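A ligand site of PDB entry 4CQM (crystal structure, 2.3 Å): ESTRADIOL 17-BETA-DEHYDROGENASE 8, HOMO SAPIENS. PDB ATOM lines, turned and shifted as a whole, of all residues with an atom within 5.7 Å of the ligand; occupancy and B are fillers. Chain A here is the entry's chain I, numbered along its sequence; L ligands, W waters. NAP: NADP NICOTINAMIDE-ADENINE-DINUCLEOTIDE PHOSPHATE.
A nitrogen (N1A) of the ligand lies close to the backbone carbonyl oxygen (O) of Ala 74 (3.5 Å). Gly 18 touches the ligand (CA to O4B, 3.5 Å). Gly 20 touches the ligand. Gly 22 touches the ligand (CA to O2N, 3.4 Å). CB of Ala 104 touches N3A of the ligand, 3.6 Å away. Ile 106 touches the ligand. CG2 of Val 126 touches N6A of the ligand, at 3.5 Å. Ile 154 touches the ligand (CG2 to O4D, 3.2 Å). Ser 155 touches the ligand. Ser 156 touches the ligand. Pro 199 touches the ligand (O to C5N, 3.3 Å). Gly 200 touches the ligand (O to C4N, 3.0 Å). Phe 201 touches the ligand (CA to O7N, 3.99 Å). CD of Pro 205 touches O2A of the ligand (3.5 Å). Met 206 touches the ligand. CG2 of Thr 207 touches O7N of the ligand (3.1 Å). Along chain A the residues within 4 Å of the ligand span positions 18 to 207. The nearest printed residue that does not touch the ligand is Asp 44 (4.2 Å).
The side-chain hydroxyl (OG) of Ser 21 is in hydrogen-bond range of an oxygen (O2A) of the ligand (2.8 Å). The side-chain hydroxyl (OG1) of Thr 204 lies within hydrogen-bond range of an oxygen (O1N) of the ligand, at 2.6 Å. The backbone NH (N) of Ser 21 lies close to an oxygen (O3B) of the ligand, 3.4 Å away. The backbone NH of Ile 23 is in hydrogen-bond range of an oxygen (O2N) of the ligand. The backbone NH (N) of Ile 202 lies within hydrogen-bond range of an oxygen (O7N) of the ligand. The backbone NH (N) of Leu 43 sits at hydrogen-bond distance from a nitrogen (N3A) of the ligand. A nitrogen (N1A) of the ligand is in hydrogen-bond range of the backbone NH (N) of Val 76, 3.2 Å away. OD1 of Asp 75 sits at hydrogen-bond distance from N6A of the ligand (2.7 Å). OD2 of Asp 42 lies within hydrogen-bond range of O3B of the ligand, at 2.7 Å. OH of Tyr 169 sits at hydrogen-bond distance from O2D of the ligand (2.7 Å). The backbone NH (N) of Gly 105 lies close to an oxygen (O3D) of the ligand, 3.4 Å away. O2D of the ligand sits at hydrogen-bond distance from NZ of Lys 173 (2.9 Å). O of Cys 103 sits at hydrogen-bond distance from O3D of the ligand.
OD2 of Asp 42 sits at hydrogen-bond distance from N of Gly 20 (2.9 Å). N of Ile 154 is in hydrogen-bond range of O of Ser 102 (3.3 Å). The side-chain carboxylate (OD2) of Asp 75 is in hydrogen-bond range of the side-chain hydroxyl (OG) of Ser 77 (2.8 Å). The side-chain hydroxyl (OG1) of Thr 207 sits at hydrogen-bond distance from the backbone carbonyl oxygen (O) of Ile 202, 2.5 Å away. OG1 of Thr 204 lies close to N of Met 206 (3.5 Å). The side-chain hydroxyl of Ser 155 sits at hydrogen-bond distance from the backbone carbonyl oxygen of Lys 173, at 2.8 Å. N of Ile 106 sits at hydrogen-bond distance from OD1 of Asn 127 (3.0 Å). O of Thr 204 lies within hydrogen-bond range of OG1 of Thr 207 (2.7 Å).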
ATOM      1  N   THR A  17       4.231  26.312  21.043  1.00  0.00           N
ATOM      2  CA  THR A  17       3.804  24.947  21.325  1.00  0.00           C
ATOM      3  C   THR A  17       4.621  24.376  22.483  1.00  0.00           C
ATOM      4  O   THR A  17       5.805  24.647  22.604  1.00  0.00           O
ATOM      5  CB  THR A  17       3.943  24.035  20.096  1.00  0.00           C
ATOM      6  OG1 THR A  17       5.324  23.793  19.841  1.00  0.00           O
ATOM      7  CG2 THR A  17       3.303  24.690  18.878  1.00  0.00           C
ATOM      8  N   GLY A  18       3.967  23.585  23.332  1.00  0.00           N
ATOM      9  CA  GLY A  18       4.624  23.037  24.499  1.00  0.00           C
ATOM     10  C   GLY A  18       4.943  24.130  25.497  1.00  0.00           C
ATOM     11  O   GLY A  18       5.979  24.108  26.162  1.00  0.00           O
ATOM     12  N   ALA A  19       4.038  25.101  25.603  1.00  0.00           N
ATOM     13  CA  ALA A  19       4.241  26.244  26.484  1.00  0.00           C
ATOM     14  C   ALA A  19       3.732  25.986  27.886  1.00  0.00           C
ATOM     15  O   ALA A  19       3.748  26.866  28.743  1.00  0.00           O
ATOM     16  CB  ALA A  19       3.564  27.478  25.892  1.00  0.00           C
ATOM     17  N   GLY A  20       3.272  24.761  28.135  1.00  0.00           N
ATOM     18  CA  GLY A  20       2.697  24.404  29.420  1.00  0.00           C
ATOM     19  C   GLY A  20       3.729  24.090  30.488  1.00  0.00           C
ATOM     20  O   GLY A  20       3.371  23.883  31.646  1.00  0.00           O
ATOM     21  N   SER A  21       5.010  24.072  30.112  1.00  0.00           N
ATOM     22  CA  SER A  21       6.063  23.725  31.051  1.00  0.00           C
ATOM     23  C   SER A  21       7.447  24.130  30.563  1.00  0.00           C
ATOM     24  O   SER A  21       7.678  24.290  29.366  1.00  0.00           O
ATOM     25  CB  SER A  21       6.047  22.223  31.327  1.00  0.00           C
ATOM     26  OG  SER A  21       7.134  21.835  32.142  1.00  0.00           O
ATOM     27  N   GLY A  22       8.371  24.294  31.520  1.00  0.00           N
ATOM     28  CA  GLY A  22       9.774  24.499  31.234  1.00  0.00           C
ATOM     29  C   GLY A  22      10.133  25.626  30.282  1.00  0.00           C
ATOM     30  O   GLY A  22       9.790  26.785  30.508  1.00  0.00           O
ATOM     31  N   ILE A  23      10.833  25.260  29.215  1.00  0.00           N
ATOM     32  CA  ILE A  23      11.313  26.226  28.226  1.00  0.00           C
ATOM     33  C   ILE A  23      10.168  26.956  27.541  1.00  0.00           C
ATOM     34  O   ILE A  23      10.184  28.186  27.433  1.00  0.00           O
ATOM     35  CB  ILE A  23      12.190  25.544  27.164  1.00  0.00           C
ATOM     36  CG1 ILE A  23      13.428  24.922  27.813  1.00  0.00           C
ATOM     37  CG2 ILE A  23      12.589  26.532  26.080  1.00  0.00           C
ATOM     38  CD1 ILE A  23      14.352  24.228  26.838  1.00  0.00           C
ATOM     39  N   GLY A  24       9.178  26.205  27.087  1.00  0.00           N
ATOM     40  CA  GLY A  24       8.013  26.775  26.437  1.00  0.00           C
ATOM     41  C   GLY A  24       7.296  27.784  27.309  1.00  0.00           C
ATOM     42  O   GLY A  24       6.774  28.788  26.809  1.00  0.00           O
ATOM     43  N   CYS A  41       0.323  27.066  23.347  1.00  0.00           N
ATOM     44  CA  CYS A  41      -0.194  25.754  22.957  1.00  0.00           C
ATOM     45  C   CYS A  41       0.532  24.646  23.709  1.00  0.00           C
ATOM     46  O   CYS A  41       1.737  24.724  23.953  1.00  0.00           O
ATOM     47  CB  CYS A  41      -0.045  25.538  21.450  1.00  0.00           C
ATOM     48  SG  CYS A  41      -0.533  23.882  20.913  1.00  0.00           S
ATOM     49  N   ASP A  42      -0.216  23.611  24.089  1.00  0.00           N
ATOM     50  CA  ASP A  42       0.340  22.491  24.832  1.00  0.00           C
ATOM     51  C   ASP A  42      -0.603  21.299  24.781  1.00  0.00           C
ATOM     52  O   ASP A  42      -1.820  21.464  24.672  1.00  0.00           O
ATOM     53  CB  ASP A  42       0.603  22.889  26.285  1.00  0.00           C
ATOM     54  CG  ASP A  42       1.455  21.886  27.027  1.00  0.00           C
ATOM     55  OD1 ASP A  42       0.904  20.881  27.511  1.00  0.00           O
ATOM     56  OD2 ASP A  42       2.688  22.106  27.118  1.00  0.00           O
ATOM     57  N   LEU A  43      -0.048  20.099  24.851  1.00  0.00           N
ATOM     58  CA  LEU A  43      -0.851  18.868  24.859  1.00  0.00           C
ATOM     59  C   LEU A  43      -1.739  18.838  26.086  1.00  0.00           C
ATOM     60  O   LEU A  43      -2.911  18.444  26.013  1.00  0.00           O
ATOM     61  CB  LEU A  43       0.054  17.633  24.808  1.00  0.00           C
ATOM     62  CG  LEU A  43      -0.663  16.285  24.719  1.00  0.00           C
ATOM     63  CD1 LEU A  43      -1.515  16.213  23.466  1.00  0.00           C
ATOM     64  CD2 LEU A  43       0.347  15.142  24.749  1.00  0.00           C
ATOM     65  N   ASP A  44      -1.185  19.250  27.227  1.00  0.00           N
ATOM     66  CA  ASP A  44      -1.956  19.389  28.446  1.00  0.00           C
ATOM     67  C   ASP A  44      -2.540  20.795  28.506  1.00  0.00           C
ATOM     68  O   ASP A  44      -1.810  21.771  28.694  1.00  0.00           O
ATOM     69  CB  ASP A  44      -1.082  19.108  29.677  1.00  0.00           C
ATOM     70  CG  ASP A  44      -1.864  19.187  30.971  1.00  0.00           C
ATOM     71  OD1 ASP A  44      -3.108  19.080  30.943  1.00  0.00           O
ATOM     72  OD2 ASP A  44      -1.236  19.361  32.034  1.00  0.00           O
ATOM     73  N   ALA A  47      -1.997  22.747  31.672  1.00  0.00           N
ATOM     74  CA  ALA A  47      -0.669  23.327  31.759  1.00  0.00           C
ATOM     75  C   ALA A  47      -0.572  24.588  30.889  1.00  0.00           C
ATOM     76  O   ALA A  47       0.120  25.543  31.239  1.00  0.00           O
ATOM     77  CB  ALA A  47       0.383  22.313  31.347  1.00  0.00           C
ATOM     78  N   ALA A  74      -3.455  21.042  21.648  1.00  0.00           N
ATOM     79  CA  ALA A  74      -3.231  20.353  20.378  1.00  0.00           C
ATOM     80  C   ALA A  74      -2.114  19.334  20.494  1.00  0.00           C
ATOM     81  O   ALA A  74      -1.101  19.565  21.161  1.00  0.00           O
ATOM     82  CB  ALA A  74      -2.908  21.361  19.289  1.00  0.00           C
ATOM     83  N   ASP A  75      -2.297  18.187  19.839  1.00  0.00           N
ATOM     84  CA  ASP A  75      -1.252  17.189  19.729  1.00  0.00           C
ATOM     85  C   ASP A  75      -0.485  17.422  18.432  1.00  0.00           C
ATOM     86  O   ASP A  75      -0.948  17.056  17.351  1.00  0.00           O
ATOM     87  CB  ASP A  75      -1.835  15.767  19.763  1.00  0.00           C
ATOM     88  CG  ASP A  75      -0.763  14.696  19.770  1.00  0.00           C
ATOM     89  OD1 ASP A  75       0.372  14.992  20.196  1.00  0.00           O
ATOM     90  OD2 ASP A  75      -1.062  13.561  19.361  1.00  0.00           O
ATOM     91  N   VAL A  76       0.685  18.041  18.546  1.00  0.00           N
ATOM     92  CA  VAL A  76       1.441  18.492  17.382  1.00  0.00           C
ATOM     93  C   VAL A  76       1.897  17.334  16.486  1.00  0.00           C
ATOM     94  O   VAL A  76       2.272  17.554  15.331  1.00  0.00           O
ATOM     95  CB  VAL A  76       2.678  19.306  17.795  1.00  0.00           C
ATOM     96  CG1 VAL A  76       2.253  20.531  18.602  1.00  0.00           C
ATOM     97  CG2 VAL A  76       3.638  18.445  18.608  1.00  0.00           C
ATOM     98  N   SER A  77       1.841  16.117  17.008  1.00  0.00           N
ATOM     99  CA  SER A  77       2.228  14.935  16.234  1.00  0.00           C
ATOM    100  C   SER A  77       1.157  14.560  15.224  1.00  0.00           C
ATOM    101  O   SER A  77       1.416  13.818  14.277  1.00  0.00           O
ATOM    102  CB  SER A  77       2.504  13.758  17.170  1.00  0.00           C
ATOM    103  OG  SER A  77       1.339  13.383  17.886  1.00  0.00           O
ATOM    104  N   SER A 102       8.506  26.205  18.493  1.00  0.00           N
ATOM    105  CA  SER A 102       8.183  24.804  18.752  1.00  0.00           C
ATOM    106  C   SER A 102       8.979  24.250  19.925  1.00  0.00           C
ATOM    107  O   SER A 102      10.119  23.822  19.772  1.00  0.00           O
ATOM    108  CB  SER A 102       8.449  23.952  17.499  1.00  0.00           C
ATOM    109  OG  SER A 102       7.511  24.245  16.477  1.00  0.00           O
ATOM    110  N   CYS A 103       8.367  24.269  21.108  1.00  0.00           N
ATOM    111  CA  CYS A 103       9.006  23.730  22.307  1.00  0.00           C
ATOM    112  C   CYS A 103       8.393  22.388  22.695  1.00  0.00           C
ATOM    113  O   CYS A 103       8.802  21.772  23.679  1.00  0.00           O
ATOM    114  CB  CYS A 103       8.876  24.710  23.477  1.00  0.00           C
ATOM    115  SG  CYS A 103       9.542  26.351  23.143  1.00  0.00           S
ATOM    116  N   ALA A 104       7.408  21.935  21.912  1.00  0.00           N
ATOM    117  CA  ALA A 104       6.754  20.666  22.176  1.00  0.00           C
ATOM    118  C   ALA A 104       7.696  19.502  21.897  1.00  0.00           C
ATOM    119  O   ALA A 104       7.986  19.185  20.753  1.00  0.00           O
ATOM    120  CB  ALA A 104       5.496  20.535  21.322  1.00  0.00           C
ATOM    121  N   GLY A 105       8.171  18.863  22.968  1.00  0.00           N
ATOM    122  CA  GLY A 105       9.096  17.760  22.831  1.00  0.00           C
ATOM    123  C   GLY A 105       9.032  16.778  23.984  1.00  0.00           C
ATOM    124  O   GLY A 105       8.636  17.131  25.094  1.00  0.00           O
ATOM    125  N   ILE A 106       9.413  15.535  23.703  1.00  0.00           N
ATOM    126  CA  ILE A 106       9.410  14.479  24.718  1.00  0.00           C
ATOM    127  C   ILE A 106      10.691  13.660  24.655  1.00  0.00           C
ATOM    128  O   ILE A 106      11.438  13.729  23.672  1.00  0.00           O
ATOM    129  CB  ILE A 106       8.209  13.525  24.548  1.00  0.00           C
ATOM    130  CG1 ILE A 106       8.236  12.879  23.165  1.00  0.00           C
ATOM    131  CG2 ILE A 106       6.897  14.266  24.786  1.00  0.00           C
ATOM    132  CD1 ILE A 106       7.117  11.885  22.952  1.00  0.00           C
ATOM    133  N   VAL A 126       6.605  13.389  17.625  1.00  0.00           N
ATOM    134  CA  VAL A 126       6.393  14.609  18.397  1.00  0.00           C
ATOM    135  C   VAL A 126       7.477  15.655  18.136  1.00  0.00           C
ATOM    136  O   VAL A 126       7.180  16.808  17.833  1.00  0.00           O
ATOM    137  CB  VAL A 126       6.341  14.302  19.901  1.00  0.00           C
ATOM    138  CG1 VAL A 126       6.304  15.605  20.709  1.00  0.00           C
ATOM    139  CG2 VAL A 126       5.134  13.442  20.226  1.00  0.00           C
ATOM    140  N   ASN A 127       8.732  15.238  18.250  1.00  0.00           N
ATOM    141  CA  ASN A 127       9.852  16.168  18.137  1.00  0.00           C
ATOM    142  C   ASN A 127      10.175  16.549  16.686  1.00  0.00           C
ATOM    143  O   ASN A 127      10.496  17.697  16.396  1.00  0.00           O
ATOM    144  CB  ASN A 127      11.100  15.583  18.804  1.00  0.00           C
ATOM    145  CG  ASN A 127      10.883  15.263  20.261  1.00  0.00           C
ATOM    146  OD1 ASN A 127       9.755  15.295  20.757  1.00  0.00           O
ATOM    147  ND2 ASN A 127      11.963  14.957  20.971  1.00  0.00           N
ATOM    148  N   ILE A 154      13.020  24.761  18.504  1.00  0.00           N
ATOM    149  CA  ILE A 154      13.905  24.360  19.598  1.00  0.00           C
ATOM    150  C   ILE A 154      14.460  22.966  19.365  1.00  0.00           C
ATOM    151  O   ILE A 154      13.810  21.962  19.654  1.00  0.00           O
ATOM    152  CB  ILE A 154      13.181  24.393  20.957  1.00  0.00           C
ATOM    153  CG1 ILE A 154      12.489  25.742  21.154  1.00  0.00           C
ATOM    154  CG2 ILE A 154      14.160  24.124  22.074  1.00  0.00           C
ATOM    155  CD1 ILE A 154      13.432  26.912  21.170  1.00  0.00           C
ATOM    156  N   SER A 155      15.682  22.906  18.842  1.00  0.00           N
ATOM    157  CA  SER A 155      16.382  21.637  18.674  1.00  0.00           C
ATOM    158  C   SER A 155      17.080  21.255  19.977  1.00  0.00           C
ATOM    159  O   SER A 155      16.467  21.319  21.045  1.00  0.00           O
ATOM    160  CB  SER A 155      17.387  21.727  17.530  1.00  0.00           C
ATOM    161  OG  SER A 155      18.059  20.489  17.352  1.00  0.00           O
ATOM    162  N   SER A 156      18.345  20.880  19.879  1.00  0.00           N
ATOM    163  CA  SER A 156      19.156  20.562  21.048  1.00  0.00           C
ATOM    164  C   SER A 156      20.616  20.452  20.658  1.00  0.00           C
ATOM    165  O   SER A 156      20.951  20.288  19.492  1.00  0.00           O
ATOM    166  CB  SER A 156      18.682  19.266  21.706  1.00  0.00           C
ATOM    167  OG  SER A 156      19.434  18.980  22.873  1.00  0.00           O
ATOM    168  N   ILE A 157      21.504  20.535  21.651  1.00  0.00           N
ATOM    169  CA  ILE A 157      22.928  20.324  21.414  1.00  0.00           C
ATOM    170  C   ILE A 157      23.163  18.847  21.102  1.00  0.00           C
ATOM    171  O   ILE A 157      24.154  18.470  20.479  1.00  0.00           O
ATOM    172  CB  ILE A 157      23.789  20.775  22.613  1.00  0.00           C
ATOM    173  CG1 ILE A 157      25.265  20.821  22.233  1.00  0.00           C
ATOM    174  CG2 ILE A 157      23.550  19.879  23.822  1.00  0.00           C
ATOM    175  CD1 ILE A 157      25.568  21.774  21.096  1.00  0.00           C
ATOM    176  N   TYR A 169      16.033  10.546  20.192  1.00  0.00           N
ATOM    177  CA  TYR A 169      16.016  11.973  20.513  1.00  0.00           C
ATOM    178  C   TYR A 169      17.008  12.753  19.653  1.00  0.00           C
ATOM    179  O   TYR A 169      16.668  13.814  19.125  1.00  0.00           O
ATOM    180  CB  TYR A 169      16.327  12.175  21.999  1.00  0.00           C
ATOM    181  CG  TYR A 169      16.226  13.617  22.456  1.00  0.00           C
ATOM    182  CD1 TYR A 169      14.994  14.152  22.830  1.00  0.00           C
ATOM    183  CD2 TYR A 169      17.345  14.420  22.543  1.00  0.00           C
ATOM    184  CE1 TYR A 169      14.891  15.461  23.262  1.00  0.00           C
ATOM    185  CE2 TYR A 169      17.253  15.739  22.965  1.00  0.00           C
ATOM    186  CZ  TYR A 169      16.021  16.254  23.329  1.00  0.00           C
ATOM    187  OH  TYR A 169      15.922  17.551  23.753  1.00  0.00           O
ATOM    188  N   LYS A 173      16.135  15.626  16.862  1.00  0.00           N
ATOM    189  CA  LYS A 173      16.654  16.982  17.019  1.00  0.00           C
ATOM    190  C   LYS A 173      17.582  17.366  15.878  1.00  0.00           C
ATOM    191  O   LYS A 173      17.603  18.528  15.452  1.00  0.00           O
ATOM    192  CB  LYS A 173      17.381  17.112  18.358  1.00  0.00           C
ATOM    193  CG  LYS A 173      16.464  17.037  19.557  1.00  0.00           C
ATOM    194  CD  LYS A 173      15.378  18.096  19.478  1.00  0.00           C
ATOM    195  CE  LYS A 173      14.316  17.871  20.528  1.00  0.00           C
ATOM    196  NZ  LYS A 173      13.319  18.968  20.563  1.00  0.00           N
ATOM    197  N   LEU A 198      19.767  25.542  19.959  1.00  0.00           N
ATOM    198  CA  LEU A 198      20.418  24.318  20.410  1.00  0.00           C
ATOM    199  C   LEU A 198      20.838  24.431  21.879  1.00  0.00           C
ATOM    200  O   LEU A 198      21.996  24.731  22.173  1.00  0.00           O
ATOM    201  CB  LEU A 198      21.632  24.002  19.541  1.00  0.00           C
ATOM    202  CG  LEU A 198      21.429  23.270  18.207  1.00  0.00           C
ATOM    203  CD1 LEU A 198      20.628  24.112  17.225  1.00  0.00           C
ATOM    204  CD2 LEU A 198      22.776  22.880  17.613  1.00  0.00           C
ATOM    205  N   PRO A 199      19.896  24.192  22.797  1.00  0.00           N
ATOM    206  CA  PRO A 199      20.194  24.303  24.226  1.00  0.00           C
ATOM    207  C   PRO A 199      20.958  23.112  24.772  1.00  0.00           C
ATOM    208  O   PRO A 199      20.772  21.991  24.295  1.00  0.00           O
ATOM    209  CB  PRO A 199      18.793  24.389  24.868  1.00  0.00           C
ATOM    210  CG  PRO A 199      17.823  24.554  23.727  1.00  0.00           C
ATOM    211  CD  PRO A 199      18.475  23.892  22.559  1.00  0.00           C
ATOM    212  N   GLY A 200      21.820  23.359  25.756  1.00  0.00           N
ATOM    213  CA  GLY A 200      22.463  22.287  26.502  1.00  0.00           C
ATOM    214  C   GLY A 200      21.490  21.772  27.547  1.00  0.00           C
ATOM    215  O   GLY A 200      20.291  21.702  27.307  1.00  0.00           O
ATOM    216  N   PHE A 201      22.001  21.423  28.719  1.00  0.00           N
ATOM    217  CA  PHE A 201      21.136  20.967  29.803  1.00  0.00           C
ATOM    218  C   PHE A 201      20.549  22.137  30.577  1.00  0.00           C
ATOM    219  O   PHE A 201      21.270  22.982  31.104  1.00  0.00           O
ATOM    220  CB  PHE A 201      21.900  20.019  30.737  1.00  0.00           C
ATOM    221  CG  PHE A 201      22.188  18.682  30.126  1.00  0.00           C
ATOM    222  CD1 PHE A 201      23.344  18.473  29.400  1.00  0.00           C
ATOM    223  CD2 PHE A 201      21.288  17.635  30.258  1.00  0.00           C
ATOM    224  CE1 PHE A 201      23.610  17.237  28.837  1.00  0.00           C
ATOM    225  CE2 PHE A 201      21.545  16.401  29.700  1.00  0.00           C
ATOM    226  CZ  PHE A 201      22.706  16.201  28.977  1.00  0.00           C
ATOM    227  N   ILE A 202      19.217  22.172  30.648  1.00  0.00           N
ATOM    228  CA  ILE A 202      18.489  23.291  31.231  1.00  0.00           C
ATOM    229  C   ILE A 202      17.674  22.840  32.446  1.00  0.00           C
ATOM    230  O   ILE A 202      17.176  21.724  32.472  1.00  0.00           O
ATOM    231  CB  ILE A 202      17.534  23.936  30.195  1.00  0.00           C
ATOM    232  CG1 ILE A 202      18.230  24.073  28.842  1.00  0.00           C
ATOM    233  CG2 ILE A 202      17.018  25.280  30.682  1.00  0.00           C
ATOM    234  CD1 ILE A 202      19.433  25.003  28.859  1.00  0.00           C
ATOM    235  N   THR A 204      14.849  22.261  33.644  1.00  0.00           N
ATOM    236  CA  THR A 204      13.451  22.042  33.292  1.00  0.00           C
ATOM    237  C   THR A 204      13.003  20.660  33.768  1.00  0.00           C
ATOM    238  O   THR A 204      13.849  19.811  34.069  1.00  0.00           O
ATOM    239  CB  THR A 204      13.241  22.163  31.768  1.00  0.00           C
ATOM    240  OG1 THR A 204      13.865  21.065  31.094  1.00  0.00           O
ATOM    241  CG2 THR A 204      13.808  23.468  31.231  1.00  0.00           C
ATOM    242  N   PRO A 205      11.678  20.426  33.867  1.00  0.00           N
ATOM    243  CA  PRO A 205      11.148  19.103  34.244  1.00  0.00           C
ATOM    244  C   PRO A 205      11.727  17.934  33.451  1.00  0.00           C
ATOM    245  O   PRO A 205      11.732  16.813  33.951  1.00  0.00           O
ATOM    246  CB  PRO A 205       9.656  19.250  33.952  1.00  0.00           C
ATOM    247  CG  PRO A 205       9.372  20.676  34.248  1.00  0.00           C
ATOM    248  CD  PRO A 205      10.603  21.443  33.820  1.00  0.00           C
ATOM    249  N   MET A 206      12.209  18.204  32.236  1.00  0.00           N
ATOM    250  CA  MET A 206      12.829  17.161  31.430  1.00  0.00           C
ATOM    251  C   MET A 206      14.134  16.675  32.042  1.00  0.00           C
ATOM    252  O   MET A 206      14.457  15.491  31.995  1.00  0.00           O
ATOM    253  CB  MET A 206      13.071  17.673  30.001  1.00  0.00           C
ATOM    254  CG  MET A 206      13.755  16.665  29.081  1.00  0.00           C
ATOM    255  SD  MET A 206      13.865  17.227  27.374  1.00  0.00           S
ATOM    256  CE  MET A 206      12.132  17.254  26.927  1.00  0.00           C
ATOM    257  N   THR A 207      14.899  17.591  32.632  1.00  0.00           N
ATOM    258  CA  THR A 207      16.180  17.243  33.232  1.00  0.00           C
ATOM    259  C   THR A 207      16.035  16.778  34.685  1.00  0.00           C
ATOM    260  O   THR A 207      16.993  16.283  35.278  1.00  0.00           O
ATOM    261  CB  THR A 207      17.169  18.421  33.194  1.00  0.00           C
ATOM    262  OG1 THR A 207      16.522  19.609  33.643  1.00  0.00           O
ATOM    263  CG2 THR A 207      17.675  18.627  31.775  1.00  0.00           C
HETATM  264  PA  NAP L   1       9.245  20.025  29.405  1.00  0.00           P
HETATM  265  O1A NAP L   1       8.784  18.603  29.606  1.00  0.00           O
HETATM  266  O2A NAP L   1       9.329  20.966  30.592  1.00  0.00           O
HETATM  267  O5B NAP L   1       8.316  20.692  28.280  1.00  0.00           O
HETATM  268  C5B NAP L   1       7.706  19.895  27.272  1.00  0.00           C
HETATM  269  C4B NAP L   1       6.326  20.451  26.950  1.00  0.00           C
HETATM  270  O4B NAP L   1       5.906  20.028  25.653  1.00  0.00           O
HETATM  271  C3B NAP L   1       5.303  19.944  27.955  1.00  0.00           C
HETATM  272  O3B NAP L   1       4.647  21.039  28.588  1.00  0.00           O
HETATM  273  C2B NAP L   1       4.313  19.132  27.142  1.00  0.00           C
HETATM  274  O2B NAP L   1       2.964  19.405  27.545  1.00  0.00           O
HETATM  275  C1B NAP L   1       4.551  19.574  25.710  1.00  0.00           C
HETATM  276  N9A NAP L   1       4.316  18.445  24.776  1.00  0.00           N
HETATM  277  C8A NAP L   1       4.874  17.220  24.843  1.00  0.00           C
HETATM  278  N7A NAP L   1       4.438  16.424  23.837  1.00  0.00           N
HETATM  279  C5A NAP L   1       3.567  17.146  23.100  1.00  0.00           C
HETATM  280  C6A NAP L   1       2.735  16.911  21.894  1.00  0.00           C
HETATM  281  N6A NAP L   1       2.747  15.711  21.254  1.00  0.00           N
HETATM  282  N1A NAP L   1       1.968  17.929  21.454  1.00  0.00           N
HETATM  283  C2A NAP L   1       1.944  19.117  22.079  1.00  0.00           C
HETATM  284  N3A NAP L   1       2.675  19.402  23.176  1.00  0.00           N
HETATM  285  C4A NAP L   1       3.488  18.474  23.722  1.00  0.00           C
HETATM  286  O3  NAP L   1      10.676  19.986  28.664  1.00  0.00           O
HETATM  287  PN  NAP L   1      11.424  21.346  28.228  1.00  0.00           P
HETATM  288  O1N NAP L   1      12.831  21.292  28.767  1.00  0.00           O
HETATM  289  O2N NAP L   1      10.543  22.530  28.524  1.00  0.00           O
HETATM  290  O5D NAP L   1      11.505  21.141  26.638  1.00  0.00           O
HETATM  291  C5D NAP L   1      11.432  22.232  25.731  1.00  0.00           C
HETATM  292  C4D NAP L   1      12.014  21.784  24.394  1.00  0.00           C
HETATM  293  O4D NAP L   1      13.421  22.050  24.373  1.00  0.00           O
HETATM  294  C3D NAP L   1      11.831  20.285  24.225  1.00  0.00           C
HETATM  295  O3D NAP L   1      11.317  20.024  22.923  1.00  0.00           O
HETATM  296  C2D NAP L   1      13.232  19.707  24.332  1.00  0.00           C
HETATM  297  O2D NAP L   1      13.418  18.633  23.412  1.00  0.00           O
HETATM  298  C1D NAP L   1      14.144  20.873  24.004  1.00  0.00           C
HETATM  299  N1N NAP L   1      15.377  20.807  24.781  1.00  0.00           N
HETATM  300  C2N NAP L   1      15.325  20.654  26.111  1.00  0.00           C
HETATM  301  C3N NAP L   1      16.496  20.586  26.856  1.00  0.00           C
HETATM  302  C7N NAP L   1      16.439  20.407  28.348  1.00  0.00           C
HETATM  303  O7N NAP L   1      17.396  19.891  28.905  1.00  0.00           O
HETATM  304  N7N NAP L   1      15.361  20.815  29.010  1.00  0.00           N
HETATM  305  C4N NAP L   1      17.714  20.696  26.215  1.00  0.00           C
HETATM  306  C5N NAP L   1      17.751  20.864  24.839  1.00  0.00           C
HETATM  307  C6N NAP L   1      16.554  20.926  24.145  1.00  0.00           C
HETATM  308  O   HOH W   1       3.085  20.069  30.612  1.00  0.00           O
HETATM  309  O   HOH W   2       3.317  13.797  23.603  1.00  0.00           O
HETATM  310  O   HOH W   3       8.549  23.359  26.608  1.00  0.00           O
HETATM  311  O   HOH W   4      18.839  17.764  25.971  1.00  0.00           O
HETATM  312  O   HOH W   5       8.676  16.073  31.670  1.00  0.00           O
